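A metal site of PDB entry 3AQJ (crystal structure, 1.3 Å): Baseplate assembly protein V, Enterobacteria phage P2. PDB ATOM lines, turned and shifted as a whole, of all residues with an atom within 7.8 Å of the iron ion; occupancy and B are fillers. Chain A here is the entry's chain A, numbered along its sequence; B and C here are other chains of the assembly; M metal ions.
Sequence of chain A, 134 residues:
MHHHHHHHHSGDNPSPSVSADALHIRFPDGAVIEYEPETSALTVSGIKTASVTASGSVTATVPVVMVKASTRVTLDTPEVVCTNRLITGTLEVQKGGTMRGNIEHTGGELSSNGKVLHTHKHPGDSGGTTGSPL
The iron ion is bound by a ring nitrogen (NE2) of His 120 of chain A (2.2 Å). The iron ion is bound by a ring nitrogen (NE2) of His 122 of chain A, at 2.2 Å. A ring nitrogen (NE2) of His 122 of chain B binds the iron ion (2.2 Å). NE2 of His 120 of chain B binds the iron ion (2.2 Å). NE2 of His 120 of chain C binds the iron ion (2.2 Å). NE2 of His 122 of chain C is bound to the iron ion (2.3 Å).
The backbone carbonyl oxygen (O) of Leu 117 of chain A is in hydrogen-bond range of a ring nitrogen (ND1) of His 120 of chain A (2.9 Å). ND1 of His 120 of chain A sits at hydrogen-bond distance from O of Val 116 of chain A. ND1 of His 122 of chain A sits at hydrogen-bond distance from O of Gly 131 of chain B (2.8 Å). ND1 of His 122 of chain B sits at hydrogen-bond distance from O of Gly 131 of chain C (2.7 Å). ND1 of His 120 of chain B lies within hydrogen-bond range of O of Leu 117 of chain B, 2.9 Å away. The backbone carbonyl oxygen of Val 116 of chain B sits at hydrogen-bond distance from a ring nitrogen (ND1) of His 120 of chain B (3.0 Å). ND1 of His 120 of chain C lies within hydrogen-bond range of O of Val 116 of chain C (3.0 Å). O of Gly 131 of chain A lies within hydrogen-bond range of ND1 of His 122 of chain C, 2.8 Å away.
Six residues have an atom within 4 Å of the iron ion: His 120 of chain A, His 122 of chain A, His 120 of chain B, His 122 of chain B, His 120 of chain C and His 122 of chain C. The nearest printed residue that does not touch the iron ion is Pro 133 of chain C (5.2 Å).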
ATOM      1  N   VAL A 116      -6.808 -13.728  15.176  1.00  0.00           N
ATOM      2  CA  VAL A 116      -5.489 -14.220  15.611  1.00  0.00           C
ATOM      3  C   VAL A 116      -4.810 -13.145  16.435  1.00  0.00           C
ATOM      4  O   VAL A 116      -4.595 -11.993  15.941  1.00  0.00           O
ATOM      5  CB  VAL A 116      -4.651 -14.592  14.430  1.00  0.00           C
ATOM      6  CG1 VAL A 116      -3.231 -15.064  14.891  1.00  0.00           C
ATOM      7  CG2 VAL A 116      -5.328 -15.770  13.602  1.00  0.00           C
ATOM      8  N   LEU A 117      -4.450 -13.437  17.664  1.00  0.00           N
ATOM      9  CA  LEU A 117      -3.869 -12.352  18.525  1.00  0.00           C
ATOM     10  C   LEU A 117      -2.654 -11.732  17.856  1.00  0.00           C
ATOM     11  O   LEU A 117      -2.581 -10.474  17.808  1.00  0.00           O
ATOM     12  CB  LEU A 117      -3.565 -12.937  19.926  1.00  0.00           C
ATOM     13  CG  LEU A 117      -2.817 -11.983  20.927  1.00  0.00           C
ATOM     14  CD1 LEU A 117      -3.517 -10.577  21.009  1.00  0.00           C
ATOM     15  CD2 LEU A 117      -2.761 -12.565  22.289  1.00  0.00           C
ATOM     16  N   HIS A 120      -3.702 -10.036  13.934  1.00  0.00           N
ATOM     17  CA  HIS A 120      -4.959  -9.364  13.524  1.00  0.00           C
ATOM     18  C   HIS A 120      -4.770  -7.894  13.258  1.00  0.00           C
ATOM     19  O   HIS A 120      -3.920  -7.224  13.837  1.00  0.00           O
ATOM     20  CB  HIS A 120      -6.082  -9.549  14.559  1.00  0.00           C
ATOM     21  CG  HIS A 120      -5.872  -8.725  15.808  1.00  0.00           C
ATOM     22  ND1 HIS A 120      -4.973  -9.076  16.809  1.00  0.00           N
ATOM     23  CD2 HIS A 120      -6.462  -7.571  16.221  1.00  0.00           C
ATOM     24  CE1 HIS A 120      -4.966  -8.108  17.735  1.00  0.00           C
ATOM     25  NE2 HIS A 120      -5.885  -7.185  17.419  1.00  0.00           N
ATOM     26  N   LYS A 121      -5.673  -7.377  12.432  1.00  0.00           N
ATOM     27  CA  LYS A 121      -5.739  -5.940  12.100  1.00  0.00           C
ATOM     28  C   LYS A 121      -7.153  -5.481  12.376  1.00  0.00           C
ATOM     29  O   LYS A 121      -8.069  -6.276  12.606  1.00  0.00           O
ATOM     30  CB  LYS A 121      -5.393  -5.713  10.591  1.00  0.00           C
ATOM     31  CG  LYS A 121      -4.019  -6.184  10.250  1.00  0.00           C
ATOM     32  CD  LYS A 121      -3.627  -5.786   8.784  1.00  0.00           C
ATOM     33  CE  LYS A 121      -2.164  -5.984   8.458  1.00  0.00           C
ATOM     34  NZ  LYS A 121      -1.834  -5.595   7.008  1.00  0.00           N
ATOM     35  N   HIS A 122      -7.389  -4.164  12.312  1.00  0.00           N
ATOM     36  CA  HIS A 122      -8.727  -3.609  12.491  1.00  0.00           C
ATOM     37  C   HIS A 122      -8.960  -2.545  11.421  1.00  0.00           C
ATOM     38  O   HIS A 122      -8.002  -1.954  10.935  1.00  0.00           O
ATOM     39  CB  HIS A 122      -8.805  -2.768  13.835  1.00  0.00           C
ATOM     40  CG  HIS A 122      -8.488  -3.565  15.078  1.00  0.00           C
ATOM     41  ND1 HIS A 122      -9.480  -3.978  15.926  1.00  0.00           N
ATOM     42  CD2 HIS A 122      -7.287  -4.000  15.624  1.00  0.00           C
ATOM     43  CE1 HIS A 122      -8.890  -4.652  16.943  1.00  0.00           C
ATOM     44  NE2 HIS A 122      -7.579  -4.665  16.771  1.00  0.00           N
ATOM     45  N   THR A 130      -5.627  -0.738  10.100  1.00  0.00           N
ATOM     46  CA  THR A 130      -4.426  -0.699  10.938  1.00  0.00           C
ATOM     47  C   THR A 130      -3.365  -1.717  10.486  1.00  0.00           C
ATOM     48  O   THR A 130      -3.683  -2.626   9.687  1.00  0.00           O
ATOM     49  CB  THR A 130      -4.754  -0.959  12.402  1.00  0.00           C
ATOM     50  OG1 THR A 130      -5.073  -2.396  12.593  1.00  0.00           O
ATOM     51  CG2 THR A 130      -5.931  -0.156  12.943  1.00  0.00           C
ATOM     52  N   GLY A 131      -2.178  -1.626  11.021  1.00  0.00           N
ATOM     53  CA  GLY A 131      -1.221  -2.725  10.863  1.00  0.00           C
ATOM     54  C   GLY A 131      -1.527  -3.822  11.880  1.00  0.00           C
ATOM     55  O   GLY A 131      -2.513  -3.758  12.645  1.00  0.00           O
ATOM     56  N   SER A 132      -0.755  -4.880  11.875  1.00  0.00           N
ATOM     57  CA  SER A 132      -0.812  -5.937  12.869  1.00  0.00           C
ATOM     58  C   SER A 132      -0.212  -5.397  14.198  1.00  0.00           C
ATOM     59  O   SER A 132       0.361  -4.307  14.182  1.00  0.00           O
ATOM     60  CB  SER A 132       0.049  -7.116  12.379  1.00  0.00           C
ATOM     61  OG  SER A 132       1.312  -6.760  11.927  1.00  0.00           O
ATOM     62  N   PRO A 133      -0.363  -6.119  15.285  1.00  0.00           N
ATOM     63  CA  PRO A 133       0.114  -5.536  16.544  1.00  0.00           C
ATOM     64  C   PRO A 133       1.560  -5.230  16.579  1.00  0.00           C
ATOM     65  O   PRO A 133       2.453  -5.927  16.065  1.00  0.00           O
ATOM     66  CB  PRO A 133      -0.169  -6.699  17.507  1.00  0.00           C
ATOM     67  CG  PRO A 133      -1.371  -7.410  16.938  1.00  0.00           C
ATOM     68  CD  PRO A 133      -1.068  -7.410  15.452  1.00  0.00           C
ATOM     69  N   VAL B 116     -11.349  -8.450  25.112  1.00  0.00           N
ATOM     70  CA  VAL B 116     -11.803  -9.674  24.455  1.00  0.00           C
ATOM     71  C   VAL B 116     -11.144  -9.789  23.097  1.00  0.00           C
ATOM     72  O   VAL B 116     -11.200  -8.877  22.260  1.00  0.00           O
ATOM     73  CB  VAL B 116     -13.347  -9.596  24.286  1.00  0.00           C
ATOM     74  CG1 VAL B 116     -13.830 -10.834  23.521  1.00  0.00           C
ATOM     75  CG2 VAL B 116     -14.019  -9.546  25.673  1.00  0.00           C
ATOM     76  N   LEU B 117     -10.491 -10.928  22.830  1.00  0.00           N
ATOM     77  CA  LEU B 117      -9.758 -11.029  21.627  1.00  0.00           C
ATOM     78  C   LEU B 117     -10.604 -10.797  20.400  1.00  0.00           C
ATOM     79  O   LEU B 117     -10.228 -10.032  19.491  1.00  0.00           O
ATOM     80  CB  LEU B 117      -9.040 -12.445  21.546  1.00  0.00           C
ATOM     81  CG  LEU B 117      -8.338 -12.775  20.254  1.00  0.00           C
ATOM     82  CD1 LEU B 117      -7.376 -11.668  19.780  1.00  0.00           C
ATOM     83  CD2 LEU B 117      -7.515 -14.116  20.429  1.00  0.00           C
ATOM     84  N   HIS B 120     -12.587  -6.851  20.456  1.00  0.00           N
ATOM     85  CA  HIS B 120     -12.061  -5.559  21.005  1.00  0.00           C
ATOM     86  C   HIS B 120     -11.866  -4.565  19.887  1.00  0.00           C
ATOM     87  O   HIS B 120     -11.476  -4.861  18.721  1.00  0.00           O
ATOM     88  CB  HIS B 120     -10.743  -5.748  21.768  1.00  0.00           C
ATOM     89  CG  HIS B 120      -9.594  -6.103  20.900  1.00  0.00           C
ATOM     90  ND1 HIS B 120      -9.372  -7.374  20.379  1.00  0.00           N
ATOM     91  CD2 HIS B 120      -8.608  -5.312  20.395  1.00  0.00           C
ATOM     92  CE1 HIS B 120      -8.297  -7.292  19.581  1.00  0.00           C
ATOM     93  NE2 HIS B 120      -7.791  -6.051  19.595  1.00  0.00           N
ATOM     94  N   LYS B 121     -12.040  -3.292  20.267  1.00  0.00           N
ATOM     95  CA  LYS B 121     -11.686  -2.141  19.503  1.00  0.00           C
ATOM     96  C   LYS B 121     -10.563  -1.363  20.192  1.00  0.00           C
ATOM     97  O   LYS B 121     -10.237  -1.658  21.352  1.00  0.00           O
ATOM     98  CB  LYS B 121     -12.915  -1.221  19.339  1.00  0.00           C
ATOM     99  CG  LYS B 121     -13.913  -1.817  18.310  1.00  0.00           C
ATOM    100  CD  LYS B 121     -15.244  -1.204  18.584  1.00  0.00           C
ATOM    101  CE  LYS B 121     -16.194  -1.837  17.605  1.00  0.00           C
ATOM    102  NZ  LYS B 121     -17.392  -0.979  17.623  1.00  0.00           N
ATOM    103  N   HIS B 122      -9.996  -0.405  19.496  1.00  0.00           N
ATOM    104  CA  HIS B 122      -8.954   0.494  20.044  1.00  0.00           C
ATOM    105  C   HIS B 122      -9.387   1.923  19.744  1.00  0.00           C
ATOM    106  O   HIS B 122      -9.948   2.207  18.702  1.00  0.00           O
ATOM    107  CB  HIS B 122      -7.595   0.262  19.347  1.00  0.00           C
ATOM    108  CG  HIS B 122      -7.043  -1.141  19.481  1.00  0.00           C
ATOM    109  ND1 HIS B 122      -5.963  -1.413  20.315  1.00  0.00           N
ATOM    110  CD2 HIS B 122      -7.327  -2.281  18.801  1.00  0.00           C
ATOM    111  CE1 HIS B 122      -5.632  -2.707  20.110  1.00  0.00           C
ATOM    112  NE2 HIS B 122      -6.480  -3.273  19.247  1.00  0.00           N
ATOM    113  N   THR B 130     -11.286   2.403  16.274  1.00  0.00           N
ATOM    114  CA  THR B 130     -11.221   1.356  15.245  1.00  0.00           C
ATOM    115  C   THR B 130     -12.461   0.523  15.226  1.00  0.00           C
ATOM    116  O   THR B 130     -13.283   0.535  16.110  1.00  0.00           O
ATOM    117  CB  THR B 130      -9.971   0.433  15.472  1.00  0.00           C
ATOM    118  OG1 THR B 130     -10.202  -0.395  16.585  1.00  0.00           O
ATOM    119  CG2 THR B 130      -8.673   1.231  15.679  1.00  0.00           C
ATOM    120  N   GLY B 131     -12.536  -0.301  14.168  1.00  0.00           N
ATOM    121  CA  GLY B 131     -13.505  -1.411  14.163  1.00  0.00           C
ATOM    122  C   GLY B 131     -12.980  -2.550  15.006  1.00  0.00           C
ATOM    123  O   GLY B 131     -11.805  -2.524  15.548  1.00  0.00           O
ATOM    124  N   SER B 132     -13.751  -3.605  15.125  1.00  0.00           N
ATOM    125  CA  SER B 132     -13.331  -4.859  15.752  1.00  0.00           C
ATOM    126  C   SER B 132     -12.339  -5.573  14.796  1.00  0.00           C
ATOM    127  O   SER B 132     -12.090  -5.177  13.711  1.00  0.00           O
ATOM    128  CB  SER B 132     -14.557  -5.701  16.073  1.00  0.00           C
ATOM    129  OG  SER B 132     -15.315  -5.142  17.120  1.00  0.00           O
ATOM    130  N   PRO B 133     -11.749  -6.705  15.307  1.00  0.00           N
ATOM    131  CA  PRO B 133     -10.701  -7.329  14.513  1.00  0.00           C
ATOM    132  C   PRO B 133     -11.200  -7.913  13.181  1.00  0.00           C
ATOM    133  O   PRO B 133     -12.276  -8.566  13.178  1.00  0.00           O
ATOM    134  CB  PRO B 133     -10.233  -8.467  15.444  1.00  0.00           C
ATOM    135  CG  PRO B 133     -10.501  -8.023  16.811  1.00  0.00           C
ATOM    136  CD  PRO B 133     -11.836  -7.277  16.683  1.00  0.00           C
ATOM    137  N   VAL C 116       0.502  -8.669  23.423  1.00  0.00           N
ATOM    138  CA  VAL C 116      -0.225  -8.852  24.684  1.00  0.00           C
ATOM    139  C   VAL C 116      -1.694  -8.487  24.451  1.00  0.00           C
ATOM    140  O   VAL C 116      -2.008  -7.368  23.988  1.00  0.00           O
ATOM    141  CB  VAL C 116       0.393  -7.966  25.783  1.00  0.00           C
ATOM    142  CG1 VAL C 116      -0.434  -8.082  27.070  1.00  0.00           C
ATOM    143  CG2 VAL C 116       1.848  -8.336  26.065  1.00  0.00           C
ATOM    144  N   LEU C 117      -2.606  -9.376  24.794  1.00  0.00           N
ATOM    145  CA  LEU C 117      -4.010  -9.081  24.564  1.00  0.00           C
ATOM    146  C   LEU C 117      -4.453  -7.772  25.192  1.00  0.00           C
ATOM    147  O   LEU C 117      -5.059  -6.932  24.484  1.00  0.00           O
ATOM    148  CB  LEU C 117      -4.836 -10.315  25.006  1.00  0.00           C
ATOM    149  CG  LEU C 117      -6.345 -10.108  24.811  1.00  0.00           C
ATOM    150  CD1 LEU C 117      -6.807  -9.565  23.404  1.00  0.00           C
ATOM    151  CD2 LEU C 117      -7.051 -11.440  25.115  1.00  0.00           C
ATOM    152  N   HIS C 120      -1.908  -4.454  23.819  1.00  0.00           N
ATOM    153  CA  HIS C 120      -1.290  -4.241  22.524  1.00  0.00           C
ATOM    154  C   HIS C 120      -1.912  -3.026  21.800  1.00  0.00           C
ATOM    155  O   HIS C 120      -3.042  -2.652  22.042  1.00  0.00           O
ATOM    156  CB  HIS C 120      -1.368  -5.511  21.591  1.00  0.00           C
ATOM    157  CG  HIS C 120      -2.753  -5.759  21.049  1.00  0.00           C
ATOM    158  ND1 HIS C 120      -3.779  -6.281  21.794  1.00  0.00           N
ATOM    159  CD2 HIS C 120      -3.322  -5.389  19.875  1.00  0.00           C
ATOM    160  CE1 HIS C 120      -4.941  -6.265  21.079  1.00  0.00           C
ATOM    161  NE2 HIS C 120      -4.657  -5.762  19.900  1.00  0.00           N
ATOM    162  N   LYS C 121      -1.106  -2.540  20.873  1.00  0.00           N
ATOM    163  CA  LYS C 121      -1.551  -1.508  19.956  1.00  0.00           C
ATOM    164  C   LYS C 121      -1.112  -1.823  18.558  1.00  0.00           C
ATOM    165  O   LYS C 121      -0.411  -2.829  18.382  1.00  0.00           O
ATOM    166  CB  LYS C 121      -1.087  -0.123  20.425  1.00  0.00           C
ATOM    167  CG  LYS C 121       0.339  -0.061  20.595  1.00  0.00           C
ATOM    168  CD  LYS C 121       0.870   1.461  20.601  1.00  0.00           C
ATOM    169  CE  LYS C 121       0.241   2.323  21.621  1.00  0.00           C
ATOM    170  NZ  LYS C 121       0.628   3.739  21.435  1.00  0.00           N
ATOM    171  N   HIS C 122      -1.583  -1.053  17.588  1.00  0.00           N
ATOM    172  CA  HIS C 122      -1.293  -1.309  16.174  1.00  0.00           C
ATOM    173  C   HIS C 122      -0.784  -0.014  15.563  1.00  0.00           C
ATOM    174  O   HIS C 122      -1.196   1.091  15.970  1.00  0.00           O
ATOM    175  CB  HIS C 122      -2.594  -1.659  15.448  1.00  0.00           C
ATOM    176  CG  HIS C 122      -3.306  -2.871  15.957  1.00  0.00           C
ATOM    177  ND1 HIS C 122      -3.254  -4.102  15.311  1.00  0.00           N
ATOM    178  CD2 HIS C 122      -4.106  -3.047  17.011  1.00  0.00           C
ATOM    179  CE1 HIS C 122      -3.995  -4.940  15.984  1.00  0.00           C
ATOM    180  NE2 HIS C 122      -4.521  -4.370  17.056  1.00  0.00           N
ATOM    181  N   THR C 130      -2.615   3.237  17.226  1.00  0.00           N
ATOM    182  CA  THR C 130      -3.882   3.157  17.996  1.00  0.00           C
ATOM    183  C   THR C 130      -3.500   3.252  19.515  1.00  0.00           C
ATOM    184  O   THR C 130      -2.334   3.108  19.885  1.00  0.00           O
ATOM    185  CB  THR C 130      -4.546   1.867  17.694  1.00  0.00           C
ATOM    186  OG1 THR C 130      -3.823   0.732  18.266  1.00  0.00           O
ATOM    187  CG2 THR C 130      -4.797   1.575  16.196  1.00  0.00           C
ATOM    188  N   GLY C 131      -4.531   3.380  20.307  1.00  0.00           N
ATOM    189  CA  GLY C 131      -4.332   3.044  21.717  1.00  0.00           C
ATOM    190  C   GLY C 131      -4.421   1.548  21.940  1.00  0.00           C
ATOM    191  O   GLY C 131      -4.421   0.741  20.970  1.00  0.00           O
ATOM    192  N   SER C 132      -4.488   1.137  23.215  1.00  0.00           N
ATOM    193  CA  SER C 132      -4.698  -0.263  23.545  1.00  0.00           C
ATOM    194  C   SER C 132      -6.182  -0.641  23.524  1.00  0.00           C
ATOM    195  O   SER C 132      -7.024   0.258  23.268  1.00  0.00           O
ATOM    196  CB  SER C 132      -4.070  -0.497  24.926  1.00  0.00           C
ATOM    197  OG  SER C 132      -4.727   0.270  25.902  1.00  0.00           O
ATOM    198  N   PRO C 133      -6.537  -1.891  23.801  1.00  0.00           N
ATOM    199  CA  PRO C 133      -7.946  -2.260  23.609  1.00  0.00           C
ATOM    200  C   PRO C 133      -8.838  -1.571  24.597  1.00  0.00           C
ATOM    201  O   PRO C 133      -8.533  -1.375  25.817  1.00  0.00           O
ATOM    202  CB  PRO C 133      -7.922  -3.798  23.870  1.00  0.00           C
ATOM    203  CG  PRO C 133      -6.556  -4.202  23.406  1.00  0.00           C
ATOM    204  CD  PRO C 133      -5.647  -3.087  23.893  1.00  0.00           C
HETATM  205 FE    FE M   1      -6.162  -5.243  18.340  1.00  0.00          FE
